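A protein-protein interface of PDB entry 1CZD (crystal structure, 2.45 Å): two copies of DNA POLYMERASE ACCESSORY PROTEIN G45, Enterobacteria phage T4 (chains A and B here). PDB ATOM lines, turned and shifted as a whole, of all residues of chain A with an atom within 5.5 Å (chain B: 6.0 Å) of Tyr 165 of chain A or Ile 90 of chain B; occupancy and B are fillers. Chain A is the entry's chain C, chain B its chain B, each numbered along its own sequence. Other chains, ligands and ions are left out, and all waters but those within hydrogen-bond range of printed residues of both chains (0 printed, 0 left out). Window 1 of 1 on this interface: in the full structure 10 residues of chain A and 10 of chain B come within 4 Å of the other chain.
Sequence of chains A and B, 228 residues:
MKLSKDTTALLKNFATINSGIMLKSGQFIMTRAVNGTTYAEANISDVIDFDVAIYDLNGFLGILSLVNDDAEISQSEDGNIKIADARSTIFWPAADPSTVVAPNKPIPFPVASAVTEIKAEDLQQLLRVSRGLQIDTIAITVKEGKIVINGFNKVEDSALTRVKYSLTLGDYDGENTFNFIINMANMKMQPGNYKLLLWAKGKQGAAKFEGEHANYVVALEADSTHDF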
ATOM      1  N   ASP A 122      -4.743  35.072   2.379  1.00  0.00           N
ATOM      2  CA  ASP A 122      -4.440  33.774   1.785  1.00  0.00           C
ATOM      3  C   ASP A 122      -4.005  32.752   2.835  1.00  0.00           C
ATOM      4  O   ASP A 122      -4.294  31.568   2.707  1.00  0.00           O
ATOM      5  CB  ASP A 122      -3.354  33.943   0.722  1.00  0.00           C
ATOM      6  CG  ASP A 122      -3.859  34.680  -0.509  1.00  0.00           C
ATOM      7  OD1 ASP A 122      -3.023  35.197  -1.281  1.00  0.00           O
ATOM      8  OD2 ASP A 122      -5.091  34.734  -0.713  1.00  0.00           O
ATOM      9  N   GLN A 125      -7.179  31.742   4.470  1.00  0.00           N
ATOM     10  CA  GLN A 125      -7.942  30.803   3.656  1.00  0.00           C
ATOM     11  C   GLN A 125      -7.334  29.408   3.791  1.00  0.00           C
ATOM     12  O   GLN A 125      -8.044  28.423   4.007  1.00  0.00           O
ATOM     13  CB  GLN A 125      -7.936  31.214   2.178  1.00  0.00           C
ATOM     14  CG  GLN A 125      -9.008  30.482   1.372  1.00  0.00           C
ATOM     15  CD  GLN A 125      -8.812  30.573  -0.127  1.00  0.00           C
ATOM     16  OE1 GLN A 125      -7.798  30.131  -0.653  1.00  0.00           O
ATOM     17  NE2 GLN A 125      -9.789  31.139  -0.822  1.00  0.00           N
ATOM     18  N   LEU A 126      -6.016  29.340   3.660  1.00  0.00           N
ATOM     19  CA  LEU A 126      -5.297  28.087   3.771  1.00  0.00           C
ATOM     20  C   LEU A 126      -5.692  27.336   5.029  1.00  0.00           C
ATOM     21  O   LEU A 126      -6.148  26.199   4.947  1.00  0.00           O
ATOM     22  CB  LEU A 126      -3.788  28.346   3.762  1.00  0.00           C
ATOM     23  CG  LEU A 126      -2.850  27.143   3.853  1.00  0.00           C
ATOM     24  CD1 LEU A 126      -3.372  26.022   2.966  1.00  0.00           C
ATOM     25  CD2 LEU A 126      -1.447  27.556   3.415  1.00  0.00           C
ATOM     26  N   VAL A 129      -9.595  26.289   5.103  1.00  0.00           N
ATOM     27  CA  VAL A 129      -9.901  25.270   4.124  1.00  0.00           C
ATOM     28  C   VAL A 129      -9.297  23.951   4.591  1.00  0.00           C
ATOM     29  O   VAL A 129      -9.889  22.883   4.417  1.00  0.00           O
ATOM     30  CB  VAL A 129      -9.342  25.675   2.741  1.00  0.00           C
ATOM     31  CG1 VAL A 129      -9.264  24.474   1.813  1.00  0.00           C
ATOM     32  CG2 VAL A 129     -10.240  26.736   2.138  1.00  0.00           C
ATOM     33  N   LEU A 133     -11.209  20.466   4.822  1.00  0.00           N
ATOM     34  CA  LEU A 133     -10.889  19.379   3.900  1.00  0.00           C
ATOM     35  C   LEU A 133      -9.925  18.348   4.481  1.00  0.00           C
ATOM     36  O   LEU A 133      -9.266  17.611   3.741  1.00  0.00           O
ATOM     37  CB  LEU A 133     -10.299  19.949   2.605  1.00  0.00           C
ATOM     38  CG  LEU A 133     -11.132  21.036   1.913  1.00  0.00           C
ATOM     39  CD1 LEU A 133     -10.428  21.531   0.666  1.00  0.00           C
ATOM     40  CD2 LEU A 133     -12.485  20.473   1.559  1.00  0.00           C
ATOM     41  N   ILE A 135      -7.151  18.611   5.362  1.00  0.00           N
ATOM     42  CA  ILE A 135      -5.811  18.807   4.809  1.00  0.00           C
ATOM     43  C   ILE A 135      -4.849  18.855   5.984  1.00  0.00           C
ATOM     44  O   ILE A 135      -5.023  19.647   6.903  1.00  0.00           O
ATOM     45  CB  ILE A 135      -5.701  20.122   4.007  1.00  0.00           C
ATOM     46  CG1 ILE A 135      -6.530  20.013   2.725  1.00  0.00           C
ATOM     47  CG2 ILE A 135      -4.237  20.407   3.673  1.00  0.00           C
ATOM     48  CD1 ILE A 135      -6.809  21.324   2.060  1.00  0.00           C
ATOM     49  N   ILE A 149       0.954  26.381  -3.499  1.00  0.00           N
ATOM     50  CA  ILE A 149       0.887  25.541  -2.315  1.00  0.00           C
ATOM     51  C   ILE A 149      -0.256  24.555  -2.554  1.00  0.00           C
ATOM     52  O   ILE A 149      -1.384  24.966  -2.834  1.00  0.00           O
ATOM     53  CB  ILE A 149       0.585  26.359  -1.038  1.00  0.00           C
ATOM     54  CG1 ILE A 149       1.715  27.354  -0.779  1.00  0.00           C
ATOM     55  CG2 ILE A 149       0.424  25.420   0.153  1.00  0.00           C
ATOM     56  CD1 ILE A 149       1.670  28.010   0.603  1.00  0.00           C
ATOM     57  N   ASN A 150       0.032  23.259  -2.476  1.00  0.00           N
ATOM     58  CA  ASN A 150      -1.009  22.257  -2.675  1.00  0.00           C
ATOM     59  C   ASN A 150      -1.309  21.607  -1.341  1.00  0.00           C
ATOM     60  O   ASN A 150      -0.401  21.341  -0.545  1.00  0.00           O
ATOM     61  CB  ASN A 150      -0.580  21.173  -3.672  1.00  0.00           C
ATOM     62  CG  ASN A 150      -0.321  21.715  -5.054  1.00  0.00           C
ATOM     63  OD1 ASN A 150      -1.086  22.524  -5.575  1.00  0.00           O
ATOM     64  ND2 ASN A 150       0.755  21.258  -5.666  1.00  0.00           N
ATOM     65  N   GLY A 151      -2.587  21.352  -1.096  1.00  0.00           N
ATOM     66  CA  GLY A 151      -2.964  20.729   0.157  1.00  0.00           C
ATOM     67  C   GLY A 151      -3.483  19.324  -0.070  1.00  0.00           C
ATOM     68  O   GLY A 151      -4.206  19.088  -1.034  1.00  0.00           O
ATOM     69  N   VAL A 163      -4.515  16.622  -4.926  1.00  0.00           N
ATOM     70  CA  VAL A 163      -4.576  17.970  -4.378  1.00  0.00           C
ATOM     71  C   VAL A 163      -6.046  18.295  -4.090  1.00  0.00           C
ATOM     72  O   VAL A 163      -6.911  18.101  -4.935  1.00  0.00           O
ATOM     73  CB  VAL A 163      -3.944  19.014  -5.362  1.00  0.00           C
ATOM     74  CG1 VAL A 163      -4.023  18.514  -6.780  1.00  0.00           C
ATOM     75  CG2 VAL A 163      -4.656  20.351  -5.253  1.00  0.00           C
ATOM     76  N   LYS A 164      -6.325  18.770  -2.880  1.00  0.00           N
ATOM     77  CA  LYS A 164      -7.691  19.090  -2.491  1.00  0.00           C
ATOM     78  C   LYS A 164      -7.884  20.584  -2.490  1.00  0.00           C
ATOM     79  O   LYS A 164      -8.995  21.081  -2.627  1.00  0.00           O
ATOM     80  CB  LYS A 164      -7.985  18.526  -1.099  1.00  0.00           C
ATOM     81  CG  LYS A 164      -7.578  17.058  -0.937  1.00  0.00           C
ATOM     82  CD  LYS A 164      -8.054  16.464   0.389  1.00  0.00           C
ATOM     83  CE  LYS A 164      -9.576  16.414   0.456  1.00  0.00           C
ATOM     84  NZ  LYS A 164     -10.085  15.884   1.757  1.00  0.00           N
ATOM     85  N   TYR A 165      -6.778  21.295  -2.331  1.00  0.00           N
ATOM     86  CA  TYR A 165      -6.758  22.752  -2.300  1.00  0.00           C
ATOM     87  C   TYR A 165      -5.445  23.194  -2.922  1.00  0.00           C
ATOM     88  O   TYR A 165      -4.409  22.577  -2.681  1.00  0.00           O
ATOM     89  CB  TYR A 165      -6.817  23.253  -0.856  1.00  0.00           C
ATOM     90  CG  TYR A 165      -6.524  24.737  -0.684  1.00  0.00           C
ATOM     91  CD1 TYR A 165      -7.441  25.705  -1.076  1.00  0.00           C
ATOM     92  CD2 TYR A 165      -5.330  25.165  -0.102  1.00  0.00           C
ATOM     93  CE1 TYR A 165      -7.178  27.074  -0.888  1.00  0.00           C
ATOM     94  CE2 TYR A 165      -5.056  26.519   0.094  1.00  0.00           C
ATOM     95  CZ  TYR A 165      -5.981  27.466  -0.297  1.00  0.00           C
ATOM     96  OH  TYR A 165      -5.711  28.794  -0.068  1.00  0.00           O
ATOM     97  N   SER A 166      -5.485  24.248  -3.727  1.00  0.00           N
ATOM     98  CA  SER A 166      -4.267  24.761  -4.343  1.00  0.00           C
ATOM     99  C   SER A 166      -4.299  26.285  -4.261  1.00  0.00           C
ATOM    100  O   SER A 166      -5.339  26.895  -4.503  1.00  0.00           O
ATOM    101  CB  SER A 166      -4.170  24.318  -5.803  1.00  0.00           C
ATOM    102  OG  SER A 166      -2.875  24.574  -6.319  1.00  0.00           O
ATOM    103  N   LEU A 167      -3.163  26.887  -3.919  1.00  0.00           N
ATOM    104  CA  LEU A 167      -3.051  28.341  -3.775  1.00  0.00           C
ATOM    105  C   LEU A 167      -1.828  28.876  -4.525  1.00  0.00           C
ATOM    106  O   LEU A 167      -0.718  28.360  -4.368  1.00  0.00           O
ATOM    107  CB  LEU A 167      -2.941  28.697  -2.285  1.00  0.00           C
ATOM    108  CG  LEU A 167      -2.541  30.106  -1.845  1.00  0.00           C
ATOM    109  CD1 LEU A 167      -3.610  31.124  -2.259  1.00  0.00           C
ATOM    110  CD2 LEU A 167      -2.355  30.109  -0.329  1.00  0.00           C
ATOM    111  N   ILE B  63     -17.326  25.386   2.833  1.00  0.00           N
ATOM    112  CA  ILE B  63     -16.192  25.615   1.954  1.00  0.00           C
ATOM    113  C   ILE B  63     -16.428  26.839   1.062  1.00  0.00           C
ATOM    114  O   ILE B  63     -15.548  27.687   0.941  1.00  0.00           O
ATOM    115  CB  ILE B  63     -15.892  24.354   1.095  1.00  0.00           C
ATOM    116  CG1 ILE B  63     -14.924  23.447   1.849  1.00  0.00           C
ATOM    117  CG2 ILE B  63     -15.322  24.731  -0.258  1.00  0.00           C
ATOM    118  CD1 ILE B  63     -13.712  24.153   2.388  1.00  0.00           C
ATOM    119  N   LEU B  66     -15.435  30.389   2.052  1.00  0.00           N
ATOM    120  CA  LEU B  66     -14.034  30.743   2.262  1.00  0.00           C
ATOM    121  C   LEU B  66     -13.387  31.300   0.993  1.00  0.00           C
ATOM    122  O   LEU B  66     -12.207  31.660   0.991  1.00  0.00           O
ATOM    123  CB  LEU B  66     -13.250  29.527   2.762  1.00  0.00           C
ATOM    124  CG  LEU B  66     -13.819  28.842   4.008  1.00  0.00           C
ATOM    125  CD1 LEU B  66     -13.073  27.535   4.270  1.00  0.00           C
ATOM    126  CD2 LEU B  66     -13.728  29.783   5.197  1.00  0.00           C
ATOM    127  N   VAL B  67     -14.160  31.358  -0.089  1.00  0.00           N
ATOM    128  CA  VAL B  67     -13.669  31.901  -1.353  1.00  0.00           C
ATOM    129  C   VAL B  67     -14.526  33.114  -1.715  1.00  0.00           C
ATOM    130  O   VAL B  67     -15.567  33.356  -1.101  1.00  0.00           O
ATOM    131  CB  VAL B  67     -13.745  30.859  -2.503  1.00  0.00           C
ATOM    132  CG1 VAL B  67     -12.883  29.658  -2.170  1.00  0.00           C
ATOM    133  CG2 VAL B  67     -15.184  30.444  -2.742  1.00  0.00           C
ATOM    134  N   ILE B  81     -16.328  18.126  -7.890  1.00  0.00           N
ATOM    135  CA  ILE B  81     -16.569  19.562  -7.974  1.00  0.00           C
ATOM    136  C   ILE B  81     -15.298  20.379  -7.798  1.00  0.00           C
ATOM    137  O   ILE B  81     -14.463  20.088  -6.936  1.00  0.00           O
ATOM    138  CB  ILE B  81     -17.586  20.016  -6.913  1.00  0.00           C
ATOM    139  CG1 ILE B  81     -18.775  19.039  -6.877  1.00  0.00           C
ATOM    140  CG2 ILE B  81     -18.049  21.436  -7.225  1.00  0.00           C
ATOM    141  CD1 ILE B  81     -19.759  19.288  -5.750  1.00  0.00           C
ATOM    142  N   LYS B  82     -15.161  21.405  -8.625  1.00  0.00           N
ATOM    143  CA  LYS B  82     -14.003  22.285  -8.577  1.00  0.00           C
ATOM    144  C   LYS B  82     -14.515  23.686  -8.337  1.00  0.00           C
ATOM    145  O   LYS B  82     -15.365  24.180  -9.074  1.00  0.00           O
ATOM    146  CB  LYS B  82     -13.246  22.220  -9.897  1.00  0.00           C
ATOM    147  CG  LYS B  82     -12.160  23.260 -10.082  1.00  0.00           C
ATOM    148  CD  LYS B  82     -11.538  23.101 -11.467  1.00  0.00           C
ATOM    149  CE  LYS B  82     -10.463  24.144 -11.750  1.00  0.00           C
ATOM    150  NZ  LYS B  82      -9.714  23.818 -12.998  1.00  0.00           N
ATOM    151  N   ILE B  83     -14.008  24.311  -7.284  1.00  0.00           N
ATOM    152  CA  ILE B  83     -14.397  25.660  -6.905  1.00  0.00           C
ATOM    153  C   ILE B  83     -13.147  26.487  -7.114  1.00  0.00           C
ATOM    154  O   ILE B  83     -12.094  26.163  -6.581  1.00  0.00           O
ATOM    155  CB  ILE B  83     -14.809  25.715  -5.415  1.00  0.00           C
ATOM    156  CG1 ILE B  83     -15.879  24.663  -5.139  1.00  0.00           C
ATOM    157  CG2 ILE B  83     -15.308  27.103  -5.049  1.00  0.00           C
ATOM    158  CD1 ILE B  83     -16.266  24.550  -3.688  1.00  0.00           C
ATOM    159  N   ALA B  84     -13.255  27.557  -7.885  1.00  0.00           N
ATOM    160  CA  ALA B  84     -12.084  28.367  -8.155  1.00  0.00           C
ATOM    161  C   ALA B  84     -12.325  29.867  -8.189  1.00  0.00           C
ATOM    162  O   ALA B  84     -13.355  30.337  -8.660  1.00  0.00           O
ATOM    163  CB  ALA B  84     -11.465  27.922  -9.470  1.00  0.00           C
ATOM    164  N   SER B  88      -6.955  30.792  -5.972  1.00  0.00           N
ATOM    165  CA  SER B  88      -7.036  29.488  -5.310  1.00  0.00           C
ATOM    166  C   SER B  88      -8.108  28.551  -5.882  1.00  0.00           C
ATOM    167  O   SER B  88      -9.130  28.993  -6.408  1.00  0.00           O
ATOM    168  CB  SER B  88      -7.259  29.666  -3.800  1.00  0.00           C
ATOM    169  OG  SER B  88      -8.529  30.225  -3.525  1.00  0.00           O
ATOM    170  N   THR B  89      -7.854  27.249  -5.765  1.00  0.00           N
ATOM    171  CA  THR B  89      -8.760  26.224  -6.254  1.00  0.00           C
ATOM    172  C   THR B  89      -9.058  25.186  -5.178  1.00  0.00           C
ATOM    173  O   THR B  89      -8.153  24.694  -4.502  1.00  0.00           O
ATOM    174  CB  THR B  89      -8.167  25.484  -7.462  1.00  0.00           C
ATOM    175  OG1 THR B  89      -7.833  26.429  -8.488  1.00  0.00           O
ATOM    176  CG2 THR B  89      -9.178  24.482  -8.013  1.00  0.00           C
ATOM    177  N   ILE B  90     -10.336  24.851  -5.034  1.00  0.00           N
ATOM    178  CA  ILE B  90     -10.764  23.872  -4.050  1.00  0.00           C
ATOM    179  C   ILE B  90     -11.521  22.747  -4.740  1.00  0.00           C
ATOM    180  O   ILE B  90     -12.351  22.997  -5.623  1.00  0.00           O
ATOM    181  CB  ILE B  90     -11.694  24.509  -3.004  1.00  0.00           C
ATOM    182  CG1 ILE B  90     -10.961  25.630  -2.280  1.00  0.00           C
ATOM    183  CG2 ILE B  90     -12.165  23.453  -1.995  1.00  0.00           C
ATOM    184  CD1 ILE B  90     -11.833  26.357  -1.292  1.00  0.00           C
ATOM    185  N   PHE B  91     -11.233  21.512  -4.345  1.00  0.00           N
ATOM    186  CA  PHE B  91     -11.916  20.366  -4.929  1.00  0.00           C
ATOM    187  C   PHE B  91     -12.816  19.665  -3.908  1.00  0.00           C
ATOM    188  O   PHE B  91     -12.371  19.269  -2.831  1.00  0.00           O
ATOM    189  CB  PHE B  91     -10.901  19.385  -5.518  1.00  0.00           C
ATOM    190  CG  PHE B  91     -10.054  19.980  -6.617  1.00  0.00           C
ATOM    191  CD1 PHE B  91      -8.812  20.542  -6.332  1.00  0.00           C
ATOM    192  CD2 PHE B  91     -10.502  19.987  -7.934  1.00  0.00           C
ATOM    193  CE1 PHE B  91      -8.029  21.099  -7.338  1.00  0.00           C
ATOM    194  CE2 PHE B  91      -9.729  20.540  -8.949  1.00  0.00           C
ATOM    195  CZ  PHE B  91      -8.489  21.098  -8.654  1.00  0.00           C
ATOM    196  N   TRP B  92     -14.093  19.535  -4.252  1.00  0.00           N
ATOM    197  CA  TRP B  92     -15.065  18.890  -3.374  1.00  0.00           C
ATOM    198  C   TRP B  92     -15.673  17.672  -4.064  1.00  0.00           C
ATOM    199  O   TRP B  92     -16.017  17.717  -5.241  1.00  0.00           O
ATOM    200  CB  TRP B  92     -16.160  19.881  -2.981  1.00  0.00           C
ATOM    201  CG  TRP B  92     -17.007  19.404  -1.874  1.00  0.00           C
ATOM    202  CD1 TRP B  92     -18.133  18.630  -1.971  1.00  0.00           C
ATOM    203  CD2 TRP B  92     -16.812  19.655  -0.474  1.00  0.00           C
ATOM    204  NE1 TRP B  92     -18.654  18.389  -0.717  1.00  0.00           N
ATOM    205  CE2 TRP B  92     -17.862  19.005   0.219  1.00  0.00           C
ATOM    206  CE3 TRP B  92     -15.855  20.370   0.261  1.00  0.00           C
ATOM    207  CZ2 TRP B  92     -17.980  19.045   1.614  1.00  0.00           C
ATOM    208  CZ3 TRP B  92     -15.974  20.413   1.652  1.00  0.00           C
ATOM    209  CH2 TRP B  92     -17.030  19.750   2.312  1.00  0.00           C
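Among the printed residues, merely in contact across the chains: Ser 166 of chain A with Ser 88 of chain B, Tyr 165 of chain A with Thr 89 of chain B, Val 163 of chain A with Phe 91 of chain B, Leu 133 of chain A with Trp 92 of chain B, Lys 164 of chain A with Ile 90 of chain B, Val 129 of chain A with Leu 66 of chain B, Gln 125 of chain A with Val 67 of chain B, Leu 133 of chain A with Ile 90 of chain B, Tyr 165 of chain A with Ile 90 of chain B, Val 129 of chain A with Ile 90 of chain B, Leu 133 of chain A with Ile 63 of chain B and Tyr 165 of chain A with Ser 88 of chain B.
No position is printed for both chains.
O of Trp 92 of chain B sits at hydrogen-bond distance from N of Ile 81 of chain B, at 2.7 Å. The backbone carbonyl oxygen (O) of Ile 83 of chain B sits at hydrogen-bond distance from the backbone NH (N) of Ile 90 of chain B, at 2.7 Å. NZ of Lys 164 of chain A is in hydrogen-bond range of O of Leu 133 of chain A. The backbone NH (N) of Gly 151 of chain A is in hydrogen-bond range of the backbone carbonyl oxygen (O) of Tyr 165 of chain A, 2.7 Å away. OE1 of Gln 125 of chain A sits at hydrogen-bond distance from OH of Tyr 165 of chain A (2.5 Å). OD1 of Asn 150 of chain A lies within hydrogen-bond range of OG of Ser 166 of chain A (2.8 Å).
Gly 151 of chain A touches none of the printed residues of chain B. Tyr 165 of chain A touches just these residues of chain B: Ser 88, Thr 89 and Ile 90. Printed residues of chain B within 4 Å of Ser 166 of chain A: Ser 88 (3.2 Å) and Thr 89 (2.8 Å). Of the printed residues of chain A, Leu 66 of chain B touches Gln 125 and Val 129. Ala 84 of chain B touches none of the printed residues of chain A. Of the printed residues of chain A, Phe 91 of chain B touches Val 163 and Lys 164. The nearest printed residue of chain A that does not touch Ser 88 of chain B is Leu 167 of chain A (4.2 Å).
The backbone carbonyl oxygen (O) of Lys 164 of chain A is in hydrogen-bond range of the backbone NH (N) of Phe 91 of chain B, at 2.9 Å. The side-chain hydroxyl (OG) of Ser 88 of chain B is in hydrogen-bond range of the side-chain amide oxygen (OE1) of Gln 125 of chain A (3.0 Å). The backbone carbonyl oxygen (O) of Thr 89 of chain B sits at hydrogen-bond distance from the backbone NH (N) of Ser 166 of chain A (2.8 Å). O of Leu 66 of chain B lies within hydrogen-bond range of NE2 of Gln 125 of chain A (3.1 Å).
Of the 12 printed residues of chain B, 8 touch a printed residue of chain A. Printed residues of chain B that touch a printed residue of chain A: Ile 63, Leu 66, Val 67, Ser 88, Thr 89, Ile 90, Phe 91 and Trp 92. Among the printed residues, 16 pairs touch across the chains.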
